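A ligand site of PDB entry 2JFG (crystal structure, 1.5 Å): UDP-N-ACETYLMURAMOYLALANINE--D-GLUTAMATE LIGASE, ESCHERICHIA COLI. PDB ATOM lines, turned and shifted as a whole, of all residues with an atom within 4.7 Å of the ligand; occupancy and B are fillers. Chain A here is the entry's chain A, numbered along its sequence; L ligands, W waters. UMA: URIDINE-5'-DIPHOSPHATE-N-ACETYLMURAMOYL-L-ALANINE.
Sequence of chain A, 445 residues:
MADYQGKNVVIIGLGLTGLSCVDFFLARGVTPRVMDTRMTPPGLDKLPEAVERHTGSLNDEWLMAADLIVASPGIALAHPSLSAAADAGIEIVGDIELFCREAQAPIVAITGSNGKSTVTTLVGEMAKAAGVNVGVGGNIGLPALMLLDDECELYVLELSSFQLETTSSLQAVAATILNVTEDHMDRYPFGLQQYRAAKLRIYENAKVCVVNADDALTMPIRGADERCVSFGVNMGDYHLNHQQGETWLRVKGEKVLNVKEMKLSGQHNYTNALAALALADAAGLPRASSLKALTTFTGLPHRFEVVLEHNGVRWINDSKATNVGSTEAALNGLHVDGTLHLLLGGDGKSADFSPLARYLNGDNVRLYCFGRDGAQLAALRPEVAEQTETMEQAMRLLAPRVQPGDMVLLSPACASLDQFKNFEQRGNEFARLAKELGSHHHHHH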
ATOM      1  N   ILE A  12      11.815  11.798  27.932  1.00  0.00           N
ATOM      2  CA  ILE A  12      12.791  11.865  26.850  1.00  0.00           C
ATOM      3  C   ILE A  12      14.013  11.042  27.232  1.00  0.00           C
ATOM      4  O   ILE A  12      14.650  11.316  28.265  1.00  0.00           O
ATOM      5  CB  ILE A  12      13.232  13.299  26.491  1.00  0.00           C
ATOM      6  CG1 ILE A  12      12.028  14.174  26.134  1.00  0.00           C
ATOM      7  CG2 ILE A  12      14.234  13.265  25.335  1.00  0.00           C
ATOM      8  CD1 ILE A  12      12.426  15.648  26.001  1.00  0.00           C
ATOM      9  N   GLY A  13      14.317  10.052  26.400  1.00  0.00           N
ATOM     10  CA  GLY A  13      15.475   9.180  26.617  1.00  0.00           C
ATOM     11  C   GLY A  13      15.086   7.741  26.886  1.00  0.00           C
ATOM     12  O   GLY A  13      14.333   7.446  27.805  1.00  0.00           O
ATOM     13  N   GLY A  15      17.390   5.304  27.460  1.00  0.00           N
ATOM     14  CA  GLY A  15      18.558   4.662  28.059  1.00  0.00           C
ATOM     15  C   GLY A  15      18.247   4.226  29.477  1.00  0.00           C
ATOM     16  O   GLY A  15      17.087   3.996  29.841  1.00  0.00           O
ATOM     17  N   LEU A  16      19.290   4.134  30.303  1.00  0.00           N
ATOM     18  CA  LEU A  16      19.094   3.656  31.675  1.00  0.00           C
ATOM     19  C   LEU A  16      18.144   4.557  32.456  1.00  0.00           C
ATOM     20  O   LEU A  16      17.288   4.089  33.187  1.00  0.00           O
ATOM     21  CB  LEU A  16      20.427   3.550  32.426  1.00  0.00           C
ATOM     22  CG  LEU A  16      21.513   2.640  31.874  1.00  0.00           C
ATOM     23  CD1 LEU A  16      22.711   2.723  32.809  1.00  0.00           C
ATOM     24  CD2 LEU A  16      21.020   1.188  31.718  1.00  0.00           C
ATOM     25  N   THR A  17      18.314   5.875  32.324  1.00  0.00           N
ATOM     26  CA  THR A  17      17.495   6.824  33.068  1.00  0.00           C
ATOM     27  C   THR A  17      16.043   6.720  32.626  1.00  0.00           C
ATOM     28  O   THR A  17      15.124   6.651  33.449  1.00  0.00           O
ATOM     29  CB  THR A  17      17.988   8.266  32.842  1.00  0.00           C
ATOM     30  OG1 THR A  17      19.354   8.350  33.277  1.00  0.00           O
ATOM     31  CG2 THR A  17      17.142   9.239  33.657  1.00  0.00           C
ATOM     32  N   GLY A  18      15.830   6.750  31.318  1.00  0.00           N
ATOM     33  CA  GLY A  18      14.475   6.690  30.785  1.00  0.00           C
ATOM     34  C   GLY A  18      13.735   5.457  31.238  1.00  0.00           C
ATOM     35  O   GLY A  18      12.564   5.549  31.654  1.00  0.00           O
ATOM     36  N   MET A  35      10.104   9.065  24.256  1.00  0.00           N
ATOM     37  CA  MET A  35      10.716   9.396  22.984  1.00  0.00           C
ATOM     38  C   MET A  35      12.243   9.493  23.120  1.00  0.00           C
ATOM     39  O   MET A  35      12.787   9.695  24.218  1.00  0.00           O
ATOM     40  CB  MET A  35      10.168  10.720  22.457  1.00  0.00           C
ATOM     41  CG  MET A  35      10.557  11.919  23.322  1.00  0.00           C
ATOM     42  SD  MET A  35       9.864  13.435  22.636  1.00  0.00           S
ATOM     43  CE  MET A  35       8.112  13.094  22.761  1.00  0.00           C
ATOM     44  N   ASP A  36      12.943   9.379  21.998  1.00  0.00           N
ATOM     45  CA  ASP A  36      14.406   9.497  21.959  1.00  0.00           C
ATOM     46  C   ASP A  36      14.804   9.931  20.545  1.00  0.00           C
ATOM     47  O   ASP A  36      14.196   9.458  19.583  1.00  0.00           O
ATOM     48  CB  ASP A  36      15.032   8.144  22.325  1.00  0.00           C
ATOM     49  CG  ASP A  36      16.514   8.234  22.700  1.00  0.00           C
ATOM     50  OD1 ASP A  36      17.354   8.615  21.865  1.00  0.00           O
ATOM     51  OD2 ASP A  36      16.839   7.905  23.852  1.00  0.00           O
ATOM     52  N   THR A  37      15.796  10.815  20.415  1.00  0.00           N
ATOM     53  CA  THR A  37      16.225  11.228  19.070  1.00  0.00           C
ATOM     54  C   THR A  37      16.980  10.121  18.342  1.00  0.00           C
ATOM     55  O   THR A  37      17.033  10.128  17.099  1.00  0.00           O
ATOM     56  CB  THR A  37      17.094  12.509  19.045  1.00  0.00           C
ATOM     57  OG1 THR A  37      18.363  12.266  19.701  1.00  0.00           O
ATOM     58  CG2 THR A  37      16.412  13.656  19.727  1.00  0.00           C
ATOM     59  N   ARG A  38      17.579   9.198  19.102  1.00  0.00           N
ATOM     60  CA  ARG A  38      18.263   8.040  18.492  1.00  0.00           C
ATOM     61  C   ARG A  38      17.243   7.123  17.815  1.00  0.00           C
ATOM     62  O   ARG A  38      16.154   6.883  18.346  1.00  0.00           O
ATOM     63  CB  ARG A  38      19.049   7.249  19.543  1.00  0.00           C
ATOM     64  CG  ARG A  38      20.220   8.025  20.156  1.00  0.00           C
ATOM     65  CD  ARG A  38      20.799   7.338  21.395  1.00  0.00           C
ATOM     66  NE  ARG A  38      19.911   7.410  22.570  1.00  0.00           N
ATOM     67  CZ  ARG A  38      20.206   6.944  23.774  1.00  0.00           C
ATOM     68  NH1 ARG A  38      21.396   6.369  23.999  1.00  0.00           N
ATOM     69  NH2 ARG A  38      19.331   7.060  24.781  1.00  0.00           N
ATOM     70  N   LEU A  58      12.560  13.955  18.296  1.00  0.00           N
ATOM     71  CA  LEU A  58      11.600  14.295  19.337  1.00  0.00           C
ATOM     72  C   LEU A  58      10.255  14.537  18.669  1.00  0.00           C
ATOM     73  O   LEU A  58      10.212  15.118  17.572  1.00  0.00           O
ATOM     74  CB  LEU A  58      12.043  15.518  20.159  1.00  0.00           C
ATOM     75  CG  LEU A  58      13.365  15.323  20.924  1.00  0.00           C
ATOM     76  CD1 LEU A  58      13.606  16.479  21.864  1.00  0.00           C
ATOM     77  CD2 LEU A  58      13.400  13.997  21.688  1.00  0.00           C
ATOM     78  N   SER A  72      15.837  12.899  30.367  1.00  0.00           N
ATOM     79  CA  SER A  72      17.075  12.208  30.692  1.00  0.00           C
ATOM     80  C   SER A  72      18.231  13.213  30.578  1.00  0.00           C
ATOM     81  O   SER A  72      18.164  14.166  29.803  1.00  0.00           O
ATOM     82  CB  SER A  72      17.301  11.048  29.712  1.00  0.00           C
ATOM     83  OG  SER A  72      16.374  10.009  29.941  1.00  0.00           O
ATOM     84  N   PRO A  73      19.313  12.980  31.339  1.00  0.00           N
ATOM     85  CA  PRO A  73      20.423  13.957  31.270  1.00  0.00           C
ATOM     86  C   PRO A  73      21.070  14.086  29.877  1.00  0.00           C
ATOM     87  O   PRO A  73      21.707  15.100  29.589  1.00  0.00           O
ATOM     88  CB  PRO A  73      21.444  13.425  32.298  1.00  0.00           C
ATOM     89  CG  PRO A  73      21.126  11.932  32.388  1.00  0.00           C
ATOM     90  CD  PRO A  73      19.602  11.881  32.282  1.00  0.00           C
ATOM     91  N   GLY A  74      20.872  13.089  29.020  1.00  0.00           N
ATOM     92  CA  GLY A  74      21.503  13.025  27.706  1.00  0.00           C
ATOM     93  C   GLY A  74      20.812  13.865  26.629  1.00  0.00           C
ATOM     94  O   GLY A  74      21.306  13.934  25.498  1.00  0.00           O
ATOM     95  N   ILE A  75      19.685  14.501  26.952  1.00  0.00           N
ATOM     96  CA  ILE A  75      19.053  15.428  25.992  1.00  0.00           C
ATOM     97  C   ILE A  75      19.270  16.857  26.485  1.00  0.00           C
ATOM     98  O   ILE A  75      19.079  17.163  27.677  1.00  0.00           O
ATOM     99  CB  ILE A  75      17.528  15.122  25.767  1.00  0.00           C
ATOM    100  CG1 ILE A  75      16.962  15.867  24.541  1.00  0.00           C
ATOM    101  CG2 ILE A  75      16.691  15.440  27.021  1.00  0.00           C
ATOM    102  CD1 ILE A  75      17.418  15.326  23.187  1.00  0.00           C
ATOM    103  N   ASP A  95      15.215  12.886  36.253  1.00  0.00           N
ATOM    104  CA  ASP A  95      15.029  11.802  37.247  1.00  0.00           C
ATOM    105  C   ASP A  95      15.492  12.216  38.643  1.00  0.00           C
ATOM    106  O   ASP A  95      14.905  11.801  39.633  1.00  0.00           O
ATOM    107  CB  ASP A  95      15.670  10.472  36.827  1.00  0.00           C
ATOM    108  CG  ASP A  95      17.181  10.517  36.780  1.00  0.00           C
ATOM    109  OD1 ASP A  95      17.725  11.470  36.178  1.00  0.00           O
ATOM    110  OD2 ASP A  95      17.812   9.573  37.303  1.00  0.00           O
ATOM    111  N   GLY A 138      22.834   7.444  41.233  1.00  0.00           N
ATOM    112  CA  GLY A 138      22.938   8.633  40.370  1.00  0.00           C
ATOM    113  C   GLY A 138      23.866   8.378  39.197  1.00  0.00           C
ATOM    114  O   GLY A 138      23.859   7.293  38.614  1.00  0.00           O
ATOM    115  N   ASN A 139      24.653   9.396  38.847  1.00  0.00           N
ATOM    116  CA  ASN A 139      25.493   9.335  37.660  1.00  0.00           C
ATOM    117  C   ASN A 139      26.531   8.215  37.703  1.00  0.00           C
ATOM    118  O   ASN A 139      27.066   7.806  36.670  1.00  0.00           O
ATOM    119  CB  ASN A 139      26.164  10.688  37.461  1.00  0.00           C
ATOM    120  CG  ASN A 139      26.859  10.797  36.112  1.00  0.00           C
ATOM    121  OD1 ASN A 139      26.195  10.850  35.064  1.00  0.00           O
ATOM    122  ND2 ASN A 139      28.198  10.815  36.125  1.00  0.00           N
ATOM    123  N   ILE A 140      26.824   7.748  38.916  1.00  0.00           N
ATOM    124  CA  ILE A 140      27.717   6.590  39.131  1.00  0.00           C
ATOM    125  C   ILE A 140      27.238   5.325  38.386  1.00  0.00           C
ATOM    126  O   ILE A 140      28.027   4.417  38.116  1.00  0.00           O
ATOM    127  CB  ILE A 140      27.895   6.320  40.661  1.00  0.00           C
ATOM    128  CG1 ILE A 140      29.056   5.355  40.926  1.00  0.00           C
ATOM    129  CG2 ILE A 140      26.593   5.803  41.282  1.00  0.00           C
ATOM    130  CD1 ILE A 140      29.536   5.406  42.360  1.00  0.00           C
ATOM    131  N   GLY A 141      25.946   5.258  38.061  1.00  0.00           N
ATOM    132  CA  GLY A 141      25.475   4.171  37.191  1.00  0.00           C
ATOM    133  C   GLY A 141      24.240   3.400  37.640  1.00  0.00           C
ATOM    134  O   GLY A 141      23.744   2.558  36.879  1.00  0.00           O
ATOM    135  N   PRO A 143      20.589   4.211  38.538  1.00  0.00           N
ATOM    136  CA  PRO A 143      19.653   5.344  38.465  1.00  0.00           C
ATOM    137  C   PRO A 143      18.992   5.631  39.819  1.00  0.00           C
ATOM    138  O   PRO A 143      18.508   4.700  40.496  1.00  0.00           O
ATOM    139  CB  PRO A 143      18.609   4.870  37.445  1.00  0.00           C
ATOM    140  CG  PRO A 143      19.416   3.955  36.522  1.00  0.00           C
ATOM    141  CD  PRO A 143      20.313   3.215  37.478  1.00  0.00           C
ATOM    142  N   SER A 160      25.694  14.711  37.839  1.00  0.00           N
ATOM    143  CA  SER A 160      26.351  15.398  36.737  1.00  0.00           C
ATOM    144  C   SER A 160      25.785  16.811  36.580  1.00  0.00           C
ATOM    145  O   SER A 160      24.705  17.120  37.083  1.00  0.00           O
ATOM    146  CB  SER A 160      26.133  14.629  35.427  1.00  0.00           C
ATOM    147  OG  SER A 160      24.750  14.711  35.058  1.00  0.00           O
ATOM    148  N   PHE A 162      24.573  17.830  33.864  1.00  0.00           N
ATOM    149  CA  PHE A 162      23.323  17.625  33.115  1.00  0.00           C
ATOM    150  C   PHE A 162      22.142  17.381  34.052  1.00  0.00           C
ATOM    151  O   PHE A 162      21.067  17.957  33.862  1.00  0.00           O
ATOM    152  CB  PHE A 162      23.418  16.433  32.153  1.00  0.00           C
ATOM    153  CG  PHE A 162      24.520  16.534  31.126  1.00  0.00           C
ATOM    154  CD1 PHE A 162      24.997  17.767  30.647  1.00  0.00           C
ATOM    155  CD2 PHE A 162      25.026  15.354  30.564  1.00  0.00           C
ATOM    156  CE1 PHE A 162      26.008  17.820  29.678  1.00  0.00           C
ATOM    157  CE2 PHE A 162      26.027  15.404  29.582  1.00  0.00           C
ATOM    158  CZ  PHE A 162      26.502  16.625  29.143  1.00  0.00           C
ATOM    159  N   GLN A 163      22.318  16.501  35.042  1.00  0.00           N
ATOM    160  CA  GLN A 163      21.250  16.211  35.984  1.00  0.00           C
ATOM    161  C   GLN A 163      20.881  17.450  36.808  1.00  0.00           C
ATOM    162  O   GLN A 163      19.705  17.724  37.064  1.00  0.00           O
ATOM    163  CB  GLN A 163      21.687  15.066  36.921  1.00  0.00           C
ATOM    164  CG  GLN A 163      21.809  13.711  36.214  1.00  0.00           C
ATOM    165  CD  GLN A 163      22.539  12.676  37.069  1.00  0.00           C
ATOM    166  OE1 GLN A 163      23.471  13.004  37.786  1.00  0.00           O
ATOM    167  NE2 GLN A 163      22.103  11.428  36.975  1.00  0.00           N
ATOM    168  N   ASP A 183      34.770  20.196  30.379  1.00  0.00           N
ATOM    169  CA  ASP A 183      34.149  18.957  29.925  1.00  0.00           C
ATOM    170  C   ASP A 183      32.792  19.299  29.313  1.00  0.00           C
ATOM    171  O   ASP A 183      32.274  20.381  29.579  1.00  0.00           O
ATOM    172  CB  ASP A 183      33.992  17.983  31.116  1.00  0.00           C
ATOM    173  CG  ASP A 183      33.751  16.533  30.687  1.00  0.00           C
ATOM    174  OD1 ASP A 183      33.711  16.201  29.474  1.00  0.00           O
ATOM    175  OD2 ASP A 183      33.608  15.691  31.630  1.00  0.00           O
ATOM    176  N   HIS A 184      32.268  18.403  28.471  1.00  0.00           N
ATOM    177  CA  HIS A 184      30.906  18.525  27.936  1.00  0.00           C
ATOM    178  C   HIS A 184      30.681  19.796  27.158  1.00  0.00           C
ATOM    179  O   HIS A 184      29.556  20.298  27.098  1.00  0.00           O
ATOM    180  CB  HIS A 184      29.879  18.418  29.070  1.00  0.00           C
ATOM    181  CG  HIS A 184      29.979  17.142  29.841  1.00  0.00           C
ATOM    182  ND1 HIS A 184      29.841  15.912  29.247  1.00  0.00           N
ATOM    183  CD2 HIS A 184      30.258  16.910  31.144  1.00  0.00           C
ATOM    184  CE1 HIS A 184      30.003  14.961  30.157  1.00  0.00           C
ATOM    185  NE2 HIS A 184      30.244  15.539  31.325  1.00  0.00           N
ATOM    186  N   LYS A 320      37.615   5.395  32.800  1.00  0.00           N
ATOM    187  CA  LYS A 320      36.787   6.473  33.342  1.00  0.00           C
ATOM    188  C   LYS A 320      37.415   7.861  33.158  1.00  0.00           C
ATOM    189  O   LYS A 320      36.823   8.838  33.541  1.00  0.00           O
ATOM    190  CB  LYS A 320      36.497   6.234  34.822  1.00  0.00           C
ATOM    191  CG  LYS A 320      35.604   7.256  35.494  1.00  0.00           C
ATOM    192  CD  LYS A 320      34.171   7.176  35.019  1.00  0.00           C
ATOM    193  CE  LYS A 320      33.267   8.136  35.761  1.00  0.00           C
ATOM    194  NZ  LYS A 320      31.858   8.096  35.310  1.00  0.00           N
ATOM    195  N   THR A 322      37.451  10.389  31.152  1.00  0.00           N
ATOM    196  CA  THR A 322      36.611  10.778  30.026  1.00  0.00           C
ATOM    197  C   THR A 322      36.729  12.260  29.705  1.00  0.00           C
ATOM    198  O   THR A 322      35.931  12.818  28.938  1.00  0.00           O
ATOM    199  CB  THR A 322      35.128  10.471  30.322  1.00  0.00           C
ATOM    200  OG1 THR A 322      34.773  11.105  31.564  1.00  0.00           O
ATOM    201  CG2 THR A 322      34.894   8.931  30.386  1.00  0.00           C
ATOM    202  N   LEU A 417      31.029   6.661  23.615  1.00  0.00           N
ATOM    203  CA  LEU A 417      29.798   6.238  22.940  1.00  0.00           C
ATOM    204  C   LEU A 417      29.848   6.227  21.418  1.00  0.00           C
ATOM    205  O   LEU A 417      28.952   5.650  20.785  1.00  0.00           O
ATOM    206  CB  LEU A 417      28.567   6.999  23.433  1.00  0.00           C
ATOM    207  CG  LEU A 417      28.347   6.956  24.947  1.00  0.00           C
ATOM    208  CD1 LEU A 417      27.081   7.772  25.260  1.00  0.00           C
ATOM    209  CD2 LEU A 417      28.250   5.553  25.542  1.00  0.00           C
ATOM    210  N   PHE A 423      31.527   3.234  29.064  1.00  0.00           N
ATOM    211  CA  PHE A 423      32.979   3.239  29.352  1.00  0.00           C
ATOM    212  C   PHE A 423      33.424   1.920  29.998  1.00  0.00           C
ATOM    213  O   PHE A 423      34.615   1.551  29.931  1.00  0.00           O
ATOM    214  CB  PHE A 423      33.388   4.464  30.175  1.00  0.00           C
ATOM    215  CG  PHE A 423      32.933   4.404  31.605  1.00  0.00           C
ATOM    216  CD1 PHE A 423      33.620   3.631  32.534  1.00  0.00           C
ATOM    217  CD2 PHE A 423      31.794   5.099  32.008  1.00  0.00           C
ATOM    218  CE1 PHE A 423      33.198   3.567  33.857  1.00  0.00           C
ATOM    219  CE2 PHE A 423      31.356   5.021  33.324  1.00  0.00           C
ATOM    220  CZ  PHE A 423      32.058   4.255  34.248  1.00  0.00           C
HETATM  221  N1  UMA L   1      20.734  10.733  23.617  1.00  0.00           N
HETATM  222  C2  UMA L   1      20.253  11.132  22.356  1.00  0.00           C
HETATM  223  N3  UMA L   1      18.946  11.441  22.209  1.00  0.00           N
HETATM  224  C4  UMA L   1      18.085  11.332  23.244  1.00  0.00           C
HETATM  225  C5  UMA L   1      18.528  10.948  24.506  1.00  0.00           C
HETATM  226  C6  UMA L   1      19.872  10.653  24.667  1.00  0.00           C
HETATM  227  O2  UMA L   1      21.048  11.227  21.384  1.00  0.00           O
HETATM  228  O4  UMA L   1      16.876  11.591  23.064  1.00  0.00           O
HETATM  229  C1B UMA L   1      22.160  10.413  23.756  1.00  0.00           C
HETATM  230  C2B UMA L   1      22.889  11.342  24.707  1.00  0.00           C
HETATM  231  O2' UMA L   1      23.398  12.526  24.081  1.00  0.00           O
HETATM  232  C3B UMA L   1      23.970  10.488  25.307  1.00  0.00           C
HETATM  233  C4B UMA L   1      23.346   9.104  25.281  1.00  0.00           C
HETATM  234  O4B UMA L   1      22.218   9.149  24.390  1.00  0.00           O
HETATM  235  O3B UMA L   1      25.125  10.495  24.458  1.00  0.00           O
HETATM  236  C5B UMA L   1      22.893   8.627  26.650  1.00  0.00           C
HETATM  237  O5B UMA L   1      21.982   9.569  27.239  1.00  0.00           O
HETATM  238  PA  UMA L   1      20.939   9.074  28.354  1.00  0.00           P
HETATM  239  O1A UMA L   1      20.407  10.313  29.055  1.00  0.00           O
HETATM  240  O2A UMA L   1      19.989   8.063  27.830  1.00  0.00           O
HETATM  241  O3A UMA L   1      21.961   8.330  29.346  1.00  0.00           O
HETATM  242  PB  UMA L   1      21.689   7.096  30.320  1.00  0.00           P
HETATM  243  O1B UMA L   1      21.983   5.804  29.623  1.00  0.00           O
HETATM  244  O2B UMA L   1      20.364   7.312  30.976  1.00  0.00           O
HETATM  245  O1' UMA L   1      22.873   7.320  31.359  1.00  0.00           O
HETATM  246  C1' UMA L   1      22.812   8.505  32.150  1.00  0.00           C
HETATM  247  C2' UMA L   1      24.211   9.092  32.302  1.00  0.00           C
HETATM  248  N2' UMA L   1      24.662   9.513  30.975  1.00  0.00           N
HETATM  249  C7' UMA L   1      24.653  10.799  30.624  1.00  0.00           C
HETATM  250  O7' UMA L   1      24.279  11.718  31.370  1.00  0.00           O
HETATM  251  C8' UMA L   1      25.127  11.057  29.213  1.00  0.00           C
HETATM  252  C3' UMA L   1      25.097   8.025  32.943  1.00  0.00           C
HETATM  253  O3' UMA L   1      26.399   8.521  33.197  1.00  0.00           O
HETATM  254  C4' UMA L   1      24.489   7.705  34.324  1.00  0.00           C
HETATM  255  O4' UMA L   1      25.227   6.675  35.001  1.00  0.00           O
HETATM  256  C5' UMA L   1      23.020   7.269  34.242  1.00  0.00           C
HETATM  257  O5' UMA L   1      22.281   8.214  33.443  1.00  0.00           O
HETATM  258  C6' UMA L   1      22.327   7.145  35.600  1.00  0.00           C
HETATM  259  O6' UMA L   1      22.197   8.465  36.171  1.00  0.00           O
HETATM  260  C18 UMA L   1      27.351   8.246  32.175  1.00  0.00           C
HETATM  261  C19 UMA L   1      27.978   9.525  31.717  1.00  0.00           C
HETATM  262  O18 UMA L   1      28.730   9.524  30.747  1.00  0.00           O
HETATM  263  C20 UMA L   1      28.471   7.394  32.755  1.00  0.00           C
HETATM  264  N4  UMA L   1      27.680  10.624  32.391  1.00  0.00           N
HETATM  265  C21 UMA L   1      28.306  11.891  32.015  1.00  0.00           C
HETATM  266  C22 UMA L   1      29.663  11.968  32.679  1.00  0.00           C
HETATM  267  O19 UMA L   1      30.521  12.751  32.236  1.00  0.00           O
HETATM  268  O20 UMA L   1      29.898  11.242  33.671  1.00  0.00           O
HETATM  269  C23 UMA L   1      27.440  13.058  32.456  1.00  0.00           C
HETATM  270  O   HOH W   1      33.040  13.033  31.358  1.00  0.00           O
HETATM  271  O   HOH W   2      25.673   7.645  28.890  1.00  0.00           O
HETATM  272  O   HOH W   3      31.370   9.479  30.219  1.00  0.00           O
HETATM  273  O   HOH W   4      21.960   5.157  26.868  1.00  0.00           O
HETATM  274  O   HOH W   5      24.342  15.110  25.289  1.00  0.00           O
HETATM  275  O   HOH W   6      32.238   9.895  32.784  1.00  0.00           O
HETATM  276  O   HOH W   7      28.480   8.692  28.284  1.00  0.00           O
HETATM  277  O   HOH W   8      25.081   8.700  22.122  1.00  0.00           O
HETATM  278  O   HOH W   9      20.118  10.182  35.169  1.00  0.00           O
HETATM  279  O   HOH W  10      31.882  12.413  34.819  1.00  0.00           O
HETATM  280  O   HOH W  11      24.791  13.066  21.577  1.00  0.00           O
HETATM  281  O   HOH W  12      17.545   7.625  29.063  1.00  0.00           O
HETATM  282  O   HOH W  13      20.269   8.694  38.321  1.00  0.00           O
HETATM  283  O   HOH W  14      24.132  12.312  34.075  1.00  0.00           O
HETATM  284  O   HOH W  15      24.475   4.605  30.278  1.00  0.00           O
HETATM  285  O   HOH W  16      25.851   4.408  33.387  1.00  0.00           O
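O2A of the ligand lies within salt-bridge range of NH2 of Arg 38, 3.3 Å away.
An oxygen (O2') of the ligand lies within hydrogen-bond range of the backbone carbonyl oxygen of Gly 74, 2.9 Å away.
The backbone NH of Gly 141 lies close to an oxygen (O4') of the ligand.
N3 of the ligand lies close to OD1 of Asp 36, 3.3 Å away.
N3 of the ligand sits at hydrogen-bond distance from OG1 of Thr 37, 2.7 Å away.
The side-chain amide nitrogen of Gln 163 lies within hydrogen-bond range of an oxygen (O6') of the ligand.
The backbone NH of Thr 17 sits at hydrogen-bond distance from an oxygen (O2B) of the ligand.
The side-chain hydroxyl of Thr 17 lies within hydrogen-bond range of an oxygen (O2B) of the ligand (2.7 Å).
O4' of the ligand is in hydrogen-bond range of O of Asn 139, 2.7 Å away.
NE2 of His 184 is in hydrogen-bond range of O19 of the ligand (2.9 Å).
O of Gly 138 lies within hydrogen-bond range of O6' of the ligand, at 3.2 Å.
The side-chain amide oxygen of Asn 139 lies close to an oxygen (O3') of the ligand (3.0 Å).
O1A of the ligand sits at hydrogen-bond distance from N of Gly 74, 2.8 Å away.
N of Leu 16 lies within hydrogen-bond range of O1B of the ligand, at 3.2 Å.
The backbone NH (N) of Thr 37 sits at hydrogen-bond distance from an oxygen (O4) of the ligand, 3.0 Å away.
Ile 12 touches the ligand (CG2 to O4, 3.9 Å).
Gly 15 touches the ligand (CA to O2A, 3.7 Å).
Ser 72 touches the ligand (CB to O1A, 3.3 Å).
CG of Pro 73 touches O7' of the ligand, 3.3 Å away.
Ile 75 touches the ligand (CD1 to O4, 3.8 Å).
Ser 160 touches the ligand (CB to C23, 3.6 Å).
Phe 162 touches the ligand (CD2 to O7', 3.8 Å).
Leu 417 touches the ligand.
CE2 of Phe 423 touches C20 of the ligand, at 3.8 Å.
Hydrophobic or aromatic side chains within 4 Å of the ligand: Ile 12, Leu 16, Pro 73, Ile 75, Phe 162, His 184, Leu 417 and Phe 423.
Of the 30 residues printed, 20 come within 4 Å of the ligand.
Water W1 lies within hydrogen-bond range of OG1 of Thr 322, O19 of the ligand and OD2 of Asp 183.
Water W4 lies within hydrogen-bond range of an oxygen (O1B) of the ligand (2.8 Å) and the guanidinium group of Arg 38 (3.2 Å).
Water W6 lies within hydrogen-bond range of an oxygen (O20) of the ligand (2.8 Å), the side-chain hydroxyl (OG1) of Thr 322 (3.1 Å) and the side-chain amino group (NZ) of Lys 320 (3.1 Å).
Water W9 lies within hydrogen-bond range of OG1 of Thr 17 (2.7 Å), O6' of the ligand (2.9 Å), OD1 of Asp 95 (2.9 Å) and NE2 of Gln 163 (3.0 Å).
Water W13 lies within hydrogen-bond range of the side-chain carboxylate (OD2) of Asp 95 (2.8 Å) and an oxygen (O6') of the ligand (2.9 Å).
Water W5 lies within hydrogen-bond range of O2' of the ligand (3.0 Å) and O of Gly 74 (3.3 Å).
The backbone NH (N) of Ser 160 sits at hydrogen-bond distance from the side-chain amide oxygen (OE1) of Gln 163 (2.8 Å).
O of Ile 12 sits at hydrogen-bond distance from OG of Ser 72 (2.7 Å).
The backbone NH (N) of Phe 162 lies close to the side-chain hydroxyl (OG) of Ser 160, at 3.3 Å.
OD2 of Asp 36 lies within salt-bridge range of NH2 of Arg 38, at 2.8 Å.
A ring nitrogen (NE2) of His 184 sits at hydrogen-bond distance from the side-chain carboxylate (OD2) of Asp 183, at 3.4 Å.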
